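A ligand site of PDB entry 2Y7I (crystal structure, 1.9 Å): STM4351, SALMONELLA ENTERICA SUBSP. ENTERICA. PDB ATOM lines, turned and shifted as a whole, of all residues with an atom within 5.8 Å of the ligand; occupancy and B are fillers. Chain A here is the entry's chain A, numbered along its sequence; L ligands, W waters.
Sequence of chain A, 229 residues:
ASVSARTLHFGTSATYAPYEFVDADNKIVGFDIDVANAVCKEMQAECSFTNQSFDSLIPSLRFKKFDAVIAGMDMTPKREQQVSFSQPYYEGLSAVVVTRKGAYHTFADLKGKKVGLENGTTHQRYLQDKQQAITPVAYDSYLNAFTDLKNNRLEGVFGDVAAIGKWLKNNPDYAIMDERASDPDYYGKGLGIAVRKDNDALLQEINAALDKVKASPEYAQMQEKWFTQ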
ATOM      1  N   THR A  12      12.893  -0.708 -23.579  1.00  0.00           N
ATOM      2  CA  THR A  12      14.111  -0.479 -22.808  1.00  0.00           C
ATOM      3  C   THR A  12      15.176  -1.523 -23.167  1.00  0.00           C
ATOM      4  O   THR A  12      14.914  -2.491 -23.907  1.00  0.00           O
ATOM      5  CB  THR A  12      13.850  -0.499 -21.272  1.00  0.00           C
ATOM      6  OG1 THR A  12      14.957   0.120 -20.594  1.00  0.00           O
ATOM      7  CG2 THR A  12      13.670  -1.911 -20.746  1.00  0.00           C
ATOM      8  N   SER A  13      16.385  -1.325 -22.648  1.00  0.00           N
ATOM      9  CA  SER A  13      17.469  -2.280 -22.783  1.00  0.00           C
ATOM     10  C   SER A  13      17.982  -2.609 -21.395  1.00  0.00           C
ATOM     11  O   SER A  13      18.744  -1.836 -20.804  1.00  0.00           O
ATOM     12  CB  SER A  13      18.613  -1.715 -23.612  1.00  0.00           C
ATOM     13  OG  SER A  13      19.597  -2.711 -23.832  1.00  0.00           O
ATOM     14  N   ALA A  14      17.543  -3.764 -20.878  1.00  0.00           N
ATOM     15  CA  ALA A  14      17.777  -4.164 -19.489  1.00  0.00           C
ATOM     16  C   ALA A  14      19.157  -4.804 -19.277  1.00  0.00           C
ATOM     17  O   ALA A  14      19.253  -5.898 -18.729  1.00  0.00           O
ATOM     18  CB  ALA A  14      16.657  -5.100 -19.038  1.00  0.00           C
ATOM     19  N   THR A  15      20.193  -4.070 -19.677  1.00  0.00           N
ATOM     20  CA  THR A  15      21.590  -4.498 -19.652  1.00  0.00           C
ATOM     21  C   THR A  15      22.400  -3.612 -18.713  1.00  0.00           C
ATOM     22  O   THR A  15      23.643  -3.685 -18.675  1.00  0.00           O
ATOM     23  CB  THR A  15      22.200  -4.332 -21.080  1.00  0.00           C
ATOM     24  OG1 THR A  15      21.972  -2.987 -21.542  1.00  0.00           O
ATOM     25  CG2 THR A  15      21.556  -5.297 -22.055  1.00  0.00           C
ATOM     26  N   TYR A  16      21.701  -2.767 -17.955  1.00  0.00           N
ATOM     27  CA  TYR A  16      22.303  -1.548 -17.400  1.00  0.00           C
ATOM     28  C   TYR A  16      21.869  -1.238 -15.966  1.00  0.00           C
ATOM     29  O   TYR A  16      21.311  -0.180 -15.708  1.00  0.00           O
ATOM     30  CB  TYR A  16      21.965  -0.371 -18.349  1.00  0.00           C
ATOM     31  CG  TYR A  16      23.061   0.680 -18.522  1.00  0.00           C
ATOM     32  CD1 TYR A  16      24.366   0.303 -18.848  1.00  0.00           C
ATOM     33  CD2 TYR A  16      22.784   2.046 -18.371  1.00  0.00           C
ATOM     34  CE1 TYR A  16      25.372   1.264 -19.009  1.00  0.00           C
ATOM     35  CE2 TYR A  16      23.777   3.011 -18.531  1.00  0.00           C
ATOM     36  CZ  TYR A  16      25.075   2.611 -18.857  1.00  0.00           C
ATOM     37  OH  TYR A  16      26.072   3.541 -19.024  1.00  0.00           O
ATOM     38  N   TYR A  19      19.801   1.240 -13.613  1.00  0.00           N
ATOM     39  CA  TYR A  19      18.749   1.875 -14.400  1.00  0.00           C
ATOM     40  C   TYR A  19      17.671   0.850 -14.798  1.00  0.00           C
ATOM     41  O   TYR A  19      16.493   1.027 -14.502  1.00  0.00           O
ATOM     42  CB  TYR A  19      19.336   2.547 -15.648  1.00  0.00           C
ATOM     43  CG  TYR A  19      20.374   3.621 -15.347  1.00  0.00           C
ATOM     44  CD1 TYR A  19      19.975   4.919 -15.022  1.00  0.00           C
ATOM     45  CD2 TYR A  19      21.741   3.329 -15.363  1.00  0.00           C
ATOM     46  CE1 TYR A  19      20.911   5.903 -14.738  1.00  0.00           C
ATOM     47  CE2 TYR A  19      22.677   4.321 -15.090  1.00  0.00           C
ATOM     48  CZ  TYR A  19      22.259   5.586 -14.781  1.00  0.00           C
ATOM     49  OH  TYR A  19      23.178   6.566 -14.500  1.00  0.00           O
ATOM     50  N   GLU A  20      18.094  -0.229 -15.445  1.00  0.00           N
ATOM     51  CA  GLU A  20      17.213  -1.338 -15.820  1.00  0.00           C
ATOM     52  C   GLU A  20      18.055  -2.583 -16.034  1.00  0.00           C
ATOM     53  O   GLU A  20      19.114  -2.520 -16.657  1.00  0.00           O
ATOM     54  CB  GLU A  20      16.403  -1.051 -17.097  1.00  0.00           C
ATOM     55  CG  GLU A  20      17.245  -0.505 -18.264  1.00  0.00           C
ATOM     56  CD  GLU A  20      17.232   0.997 -18.297  1.00  0.00           C
ATOM     57  OE1 GLU A  20      16.193   1.568 -17.901  1.00  0.00           O
ATOM     58  OE2 GLU A  20      18.247   1.618 -18.728  1.00  0.00           O
ATOM     59  N   PHE A  54      19.951  -1.520 -26.980  1.00  0.00           N
ATOM     60  CA  PHE A  54      19.824  -0.068 -26.781  1.00  0.00           C
ATOM     61  C   PHE A  54      19.755   0.698 -28.098  1.00  0.00           C
ATOM     62  O   PHE A  54      18.951   1.633 -28.244  1.00  0.00           O
ATOM     63  CB  PHE A  54      20.980   0.482 -25.932  1.00  0.00           C
ATOM     64  CG  PHE A  54      20.902   1.980 -25.697  1.00  0.00           C
ATOM     65  CD1 PHE A  54      20.108   2.491 -24.670  1.00  0.00           C
ATOM     66  CD2 PHE A  54      21.613   2.879 -26.510  1.00  0.00           C
ATOM     67  CE1 PHE A  54      20.035   3.873 -24.441  1.00  0.00           C
ATOM     68  CE2 PHE A  54      21.547   4.264 -26.288  1.00  0.00           C
ATOM     69  CZ  PHE A  54      20.746   4.751 -25.261  1.00  0.00           C
ATOM     70  N   LEU A  57      16.303   1.021 -29.993  1.00  0.00           N
ATOM     71  CA  LEU A  57      15.151   1.593 -29.273  1.00  0.00           C
ATOM     72  C   LEU A  57      14.529   2.779 -29.994  1.00  0.00           C
ATOM     73  O   LEU A  57      13.310   2.820 -30.178  1.00  0.00           O
ATOM     74  CB  LEU A  57      15.540   1.983 -27.848  1.00  0.00           C
ATOM     75  CG  LEU A  57      15.769   0.840 -26.850  1.00  0.00           C
ATOM     76  CD1 LEU A  57      16.344   1.408 -25.571  1.00  0.00           C
ATOM     77  CD2 LEU A  57      14.488   0.034 -26.589  1.00  0.00           C
ATOM     78  N   ALA A  71      15.435   4.327 -20.804  1.00  0.00           N
ATOM     79  CA  ALA A  71      16.621   3.462 -20.835  1.00  0.00           C
ATOM     80  C   ALA A  71      17.927   4.158 -20.455  1.00  0.00           C
ATOM     81  O   ALA A  71      18.946   3.996 -21.122  1.00  0.00           O
ATOM     82  CB  ALA A  71      16.767   2.802 -22.225  1.00  0.00           C
ATOM     83  N   GLY A  72      17.899   4.934 -19.372  1.00  0.00           N
ATOM     84  CA  GLY A  72      19.056   5.722 -18.963  1.00  0.00           C
ATOM     85  C   GLY A  72      19.561   6.577 -20.113  1.00  0.00           C
ATOM     86  O   GLY A  72      20.755   6.772 -20.265  1.00  0.00           O
ATOM     87  N   MET A  73      18.620   7.123 -20.893  1.00  0.00           N
ATOM     88  CA  MET A  73      18.948   7.746 -22.184  1.00  0.00           C
ATOM     89  C   MET A  73      19.105   9.265 -22.086  1.00  0.00           C
ATOM     90  O   MET A  73      18.123   9.981 -21.844  1.00  0.00           O
ATOM     91  CB  MET A  73      17.863   7.384 -23.217  1.00  0.00           C
ATOM     92  CG  MET A  73      18.058   8.019 -24.607  1.00  0.00           C
ATOM     93  SD  MET A  73      16.792   7.575 -25.820  1.00  0.00           S
ATOM     94  CE  MET A  73      17.286   5.867 -26.192  1.00  0.00           C
ATOM     95  N   ASP A  74      20.337   9.737 -22.278  1.00  0.00           N
ATOM     96  CA  ASP A  74      20.648  11.167 -22.304  1.00  0.00           C
ATOM     97  C   ASP A  74      19.904  11.834 -23.456  1.00  0.00           C
ATOM     98  O   ASP A  74      19.860  11.298 -24.558  1.00  0.00           O
ATOM     99  CB  ASP A  74      22.157  11.399 -22.535  1.00  0.00           C
ATOM    100  CG  ASP A  74      23.020  11.001 -21.331  1.00  0.00           C
ATOM    101  OD1 ASP A  74      22.598  10.188 -20.491  1.00  0.00           O
ATOM    102  OD2 ASP A  74      24.153  11.546 -21.234  1.00  0.00           O
ATOM    103  N   THR A  76      20.287  13.875 -25.949  1.00  0.00           N
ATOM    104  CA  THR A  76      21.308  14.491 -26.797  1.00  0.00           C
ATOM    105  C   THR A  76      20.657  15.254 -27.954  1.00  0.00           C
ATOM    106  O   THR A  76      19.528  14.941 -28.345  1.00  0.00           O
ATOM    107  CB  THR A  76      22.266  13.439 -27.366  1.00  0.00           C
ATOM    108  OG1 THR A  76      21.566  12.641 -28.325  1.00  0.00           O
ATOM    109  CG2 THR A  76      22.860  12.547 -26.252  1.00  0.00           C
ATOM    110  N   ARG A  79      19.604  12.863 -30.716  1.00  0.00           N
ATOM    111  CA  ARG A  79      18.392  12.119 -30.451  1.00  0.00           C
ATOM    112  C   ARG A  79      17.166  13.029 -30.547  1.00  0.00           C
ATOM    113  O   ARG A  79      16.100  12.581 -30.966  1.00  0.00           O
ATOM    114  CB  ARG A  79      18.467  11.411 -29.109  1.00  0.00           C
ATOM    115  CG  ARG A  79      19.531  10.312 -29.095  1.00  0.00           C
ATOM    116  CD  ARG A  79      19.785   9.791 -27.697  1.00  0.00           C
ATOM    117  NE  ARG A  79      20.836   8.773 -27.712  1.00  0.00           N
ATOM    118  CZ  ARG A  79      21.556   8.452 -26.639  1.00  0.00           C
ATOM    119  NH1 ARG A  79      21.320   9.072 -25.482  1.00  0.00           N
ATOM    120  NH2 ARG A  79      22.498   7.522 -26.732  1.00  0.00           N
ATOM    121  N   GLU A 118      28.782   0.408 -25.515  1.00  0.00           N
ATOM    122  CA  GLU A 118      27.542  -0.005 -26.167  1.00  0.00           C
ATOM    123  C   GLU A 118      27.264   0.784 -27.438  1.00  0.00           C
ATOM    124  O   GLU A 118      27.464   1.995 -27.461  1.00  0.00           O
ATOM    125  CB  GLU A 118      26.373   0.173 -25.194  1.00  0.00           C
ATOM    126  CG  GLU A 118      25.183  -0.746 -25.375  1.00  0.00           C
ATOM    127  CD  GLU A 118      24.290  -0.734 -24.138  1.00  0.00           C
ATOM    128  OE1 GLU A 118      24.022   0.363 -23.650  1.00  0.00           O
ATOM    129  OE2 GLU A 118      23.917  -1.813 -23.617  1.00  0.00           O
ATOM    130  N   GLY A 120      25.325   2.871 -30.138  1.00  0.00           N
ATOM    131  CA  GLY A 120      24.250   3.871 -30.066  1.00  0.00           C
ATOM    132  C   GLY A 120      24.318   4.870 -28.912  1.00  0.00           C
ATOM    133  O   GLY A 120      23.465   5.763 -28.801  1.00  0.00           O
ATOM    134  N   THR A 121      25.357   4.742 -28.093  1.00  0.00           N
ATOM    135  CA  THR A 121      25.481   5.544 -26.864  1.00  0.00           C
ATOM    136  C   THR A 121      26.281   6.832 -27.018  1.00  0.00           C
ATOM    137  O   THR A 121      27.057   6.999 -27.975  1.00  0.00           O
ATOM    138  CB  THR A 121      26.072   4.724 -25.670  1.00  0.00           C
ATOM    139  OG1 THR A 121      27.425   4.343 -25.963  1.00  0.00           O
ATOM    140  CG2 THR A 121      25.235   3.497 -25.402  1.00  0.00           C
ATOM    141  N   THR A 122      26.110   7.728 -26.051  1.00  0.00           N
ATOM    142  CA  THR A 122      26.967   8.898 -25.868  1.00  0.00           C
ATOM    143  C   THR A 122      28.422   8.471 -25.770  1.00  0.00           C
ATOM    144  O   THR A 122      29.317   9.117 -26.327  1.00  0.00           O
ATOM    145  CB  THR A 122      26.616   9.623 -24.558  1.00  0.00           C
ATOM    146  OG1 THR A 122      26.529   8.650 -23.512  1.00  0.00           O
ATOM    147  CG2 THR A 122      25.249  10.301 -24.671  1.00  0.00           C
ATOM    148  N   HIS A 123      28.660   7.377 -25.052  1.00  0.00           N
ATOM    149  CA  HIS A 123      30.001   6.879 -24.816  1.00  0.00           C
ATOM    150  C   HIS A 123      30.695   6.497 -26.102  1.00  0.00           C
ATOM    151  O   HIS A 123      31.885   6.782 -26.284  1.00  0.00           O
ATOM    152  CB  HIS A 123      29.968   5.714 -23.840  1.00  0.00           C
ATOM    153  CG  HIS A 123      29.111   5.967 -22.644  1.00  0.00           C
ATOM    154  ND1 HIS A 123      29.335   7.026 -21.794  1.00  0.00           N
ATOM    155  CD2 HIS A 123      28.002   5.342 -22.192  1.00  0.00           C
ATOM    156  CE1 HIS A 123      28.411   7.027 -20.840  1.00  0.00           C
ATOM    157  NE2 HIS A 123      27.584   6.022 -21.067  1.00  0.00           N
ATOM    158  N   TYR A 142      26.256  -4.185 -22.420  1.00  0.00           N
ATOM    159  CA  TYR A 142      27.335  -4.024 -21.448  1.00  0.00           C
ATOM    160  C   TYR A 142      27.700  -5.352 -20.785  1.00  0.00           C
ATOM    161  O   TYR A 142      28.872  -5.558 -20.442  1.00  0.00           O
ATOM    162  CB  TYR A 142      27.046  -2.868 -20.450  1.00  0.00           C
ATOM    163  CG  TYR A 142      27.469  -1.522 -21.019  1.00  0.00           C
ATOM    164  CD1 TYR A 142      28.808  -1.172 -21.088  1.00  0.00           C
ATOM    165  CD2 TYR A 142      26.525  -0.607 -21.500  1.00  0.00           C
ATOM    166  CE1 TYR A 142      29.227   0.060 -21.627  1.00  0.00           C
ATOM    167  CE2 TYR A 142      26.920   0.640 -22.029  1.00  0.00           C
ATOM    168  CZ  TYR A 142      28.280   0.958 -22.103  1.00  0.00           C
ATOM    169  OH  TYR A 142      28.696   2.162 -22.654  1.00  0.00           O
ATOM    170  N   ASP A 160      28.360   4.759 -17.979  1.00  0.00           N
ATOM    171  CA  ASP A 160      27.914   5.679 -16.914  1.00  0.00           C
ATOM    172  C   ASP A 160      28.473   5.249 -15.573  1.00  0.00           C
ATOM    173  O   ASP A 160      28.558   4.057 -15.274  1.00  0.00           O
ATOM    174  CB  ASP A 160      26.374   5.807 -16.865  1.00  0.00           C
ATOM    175  CG  ASP A 160      25.822   6.654 -18.012  1.00  0.00           C
ATOM    176  OD1 ASP A 160      25.878   7.900 -17.934  1.00  0.00           O
ATOM    177  OD2 ASP A 160      25.331   6.096 -19.000  1.00  0.00           O
ATOM    178  N   LEU A 191      18.490  12.731 -18.261  1.00  0.00           N
ATOM    179  CA  LEU A 191      17.816  11.541 -18.763  1.00  0.00           C
ATOM    180  C   LEU A 191      16.378  11.904 -19.083  1.00  0.00           C
ATOM    181  O   LEU A 191      15.741  12.657 -18.340  1.00  0.00           O
ATOM    182  CB  LEU A 191      17.851  10.412 -17.749  1.00  0.00           C
ATOM    183  CG  LEU A 191      19.217   9.954 -17.228  1.00  0.00           C
ATOM    184  CD1 LEU A 191      19.029   8.764 -16.327  1.00  0.00           C
ATOM    185  CD2 LEU A 191      20.166   9.642 -18.395  1.00  0.00           C
HETATM  186  N1  LIG L   1      23.557   7.137 -20.832  1.00  0.00           N
HETATM  187  C1  LIG L   1      24.178   6.555 -22.057  1.00  0.00           C
HETATM  188  C2  LIG L   1      23.495   7.100 -23.307  1.00  0.00           C
HETATM  189  O1  LIG L   1      23.840   6.715 -24.419  1.00  0.00           O
HETATM  190  C3  LIG L   1      24.102   5.010 -22.040  1.00  0.00           C
HETATM  191  C4  LIG L   1      22.677   4.460 -21.849  1.00  0.00           C
HETATM  192  C5  LIG L   1      22.615   2.932 -21.986  1.00  0.00           C
HETATM  193  N2  LIG L   1      21.337   2.442 -21.483  1.00  0.00           N
HETATM  194  C6  LIG L   1      20.951   1.164 -21.479  1.00  0.00           C
HETATM  195  N3  LIG L   1      21.733   0.206 -21.974  1.00  0.00           N
HETATM  196  N4  LIG L   1      19.771   0.846 -20.977  1.00  0.00           N
HETATM  197  O2  LIG L   1      22.561   7.921 -23.215  1.00  0.00           O
HETATM  198  O   HOH W   1      25.761   9.482 -21.068  1.00  0.00           O
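OD2 of Asp 160 is in salt-bridge range of N1 of the ligand (2.8 Å). N2 of the ligand sits at hydrogen-bond distance from O of Ala 71 (2.9 Å). An oxygen (O1) of the ligand sits close to the side-chain hydroxyl (OG1) of Thr 122, at 3.4 Å. A nitrogen (N4) of the ligand lies within salt-bridge range of the side-chain carboxylate (OE2) of Glu 20 (2.8 Å). The backbone carbonyl oxygen (O) of Gly 72 is in hydrogen-bond range of a nitrogen (N1) of the ligand (2.9 Å). N3 of the ligand sits at hydrogen-bond distance from OG1 of Thr 15 (3.2 Å). The backbone NH (N) of Thr 122 is in hydrogen-bond range of an oxygen (O1) of the ligand (3.0 Å). OD1 of Asp 74 is in salt-bridge range of N1 of the ligand, at 3.2 Å. OE1 of Glu 118 is in salt-bridge range of N3 of the ligand (2.8 Å). A nitrogen (N4) of the ligand lies within hydrogen-bond range of the backbone carbonyl oxygen (O) of Ser 13 (2.9 Å). An oxygen (O2) of the ligand lies within hydrogen-bond range of the backbone NH of Asp 74 (3.0 Å). NH2 of Arg 79 lies within salt-bridge range of O1 of the ligand, 2.8 Å away.
Water W1 lies within hydrogen-bond range of OD2 of Asp 74 (2.6 Å), OG1 of Thr 122 (2.7 Å) and N1 of the ligand (3.2 Å).
Tyr 16 touches the ligand. Phe 54 touches the ligand (CD1 to N2, 3.4 Å). Met 73 touches the ligand. Thr 121 touches the ligand. His 123 touches the ligand. Hydrophobic or aromatic side chains within 4 Å of the ligand: Tyr 16, Phe 54, Ala 71 and His 123. Along chain A the residues within 4 Å of the ligand span positions 13 to 160.
OG1 of Thr 121 sits close to N of His 123 (3.4 Å). The side-chain hydroxyl of Thr 12 sits at hydrogen-bond distance from the side-chain carboxylate of Glu 20, 3.3 Å away. O of Glu 118 is in hydrogen-bond range of OG1 of Thr 121 (2.8 Å). The side-chain hydroxyl of Tyr 142 sits at hydrogen-bond distance from the backbone NH of Glu 118, 3.4 Å away. NH1 of Arg 79 sits at hydrogen-bond distance from O of Asp 74, at 2.8 Å. The side-chain hydroxyl (OG) of Ser 13 lies within hydrogen-bond range of the side-chain hydroxyl (OG1) of Thr 15 (3.3 Å). N of Phe 54 lies within hydrogen-bond range of OG of Ser 13 (3.4 Å). The side-chain carboxylate (OE2) of Glu 118 lies within hydrogen-bond range of the side-chain hydroxyl (OG1) of Thr 15, 3.1 Å away.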
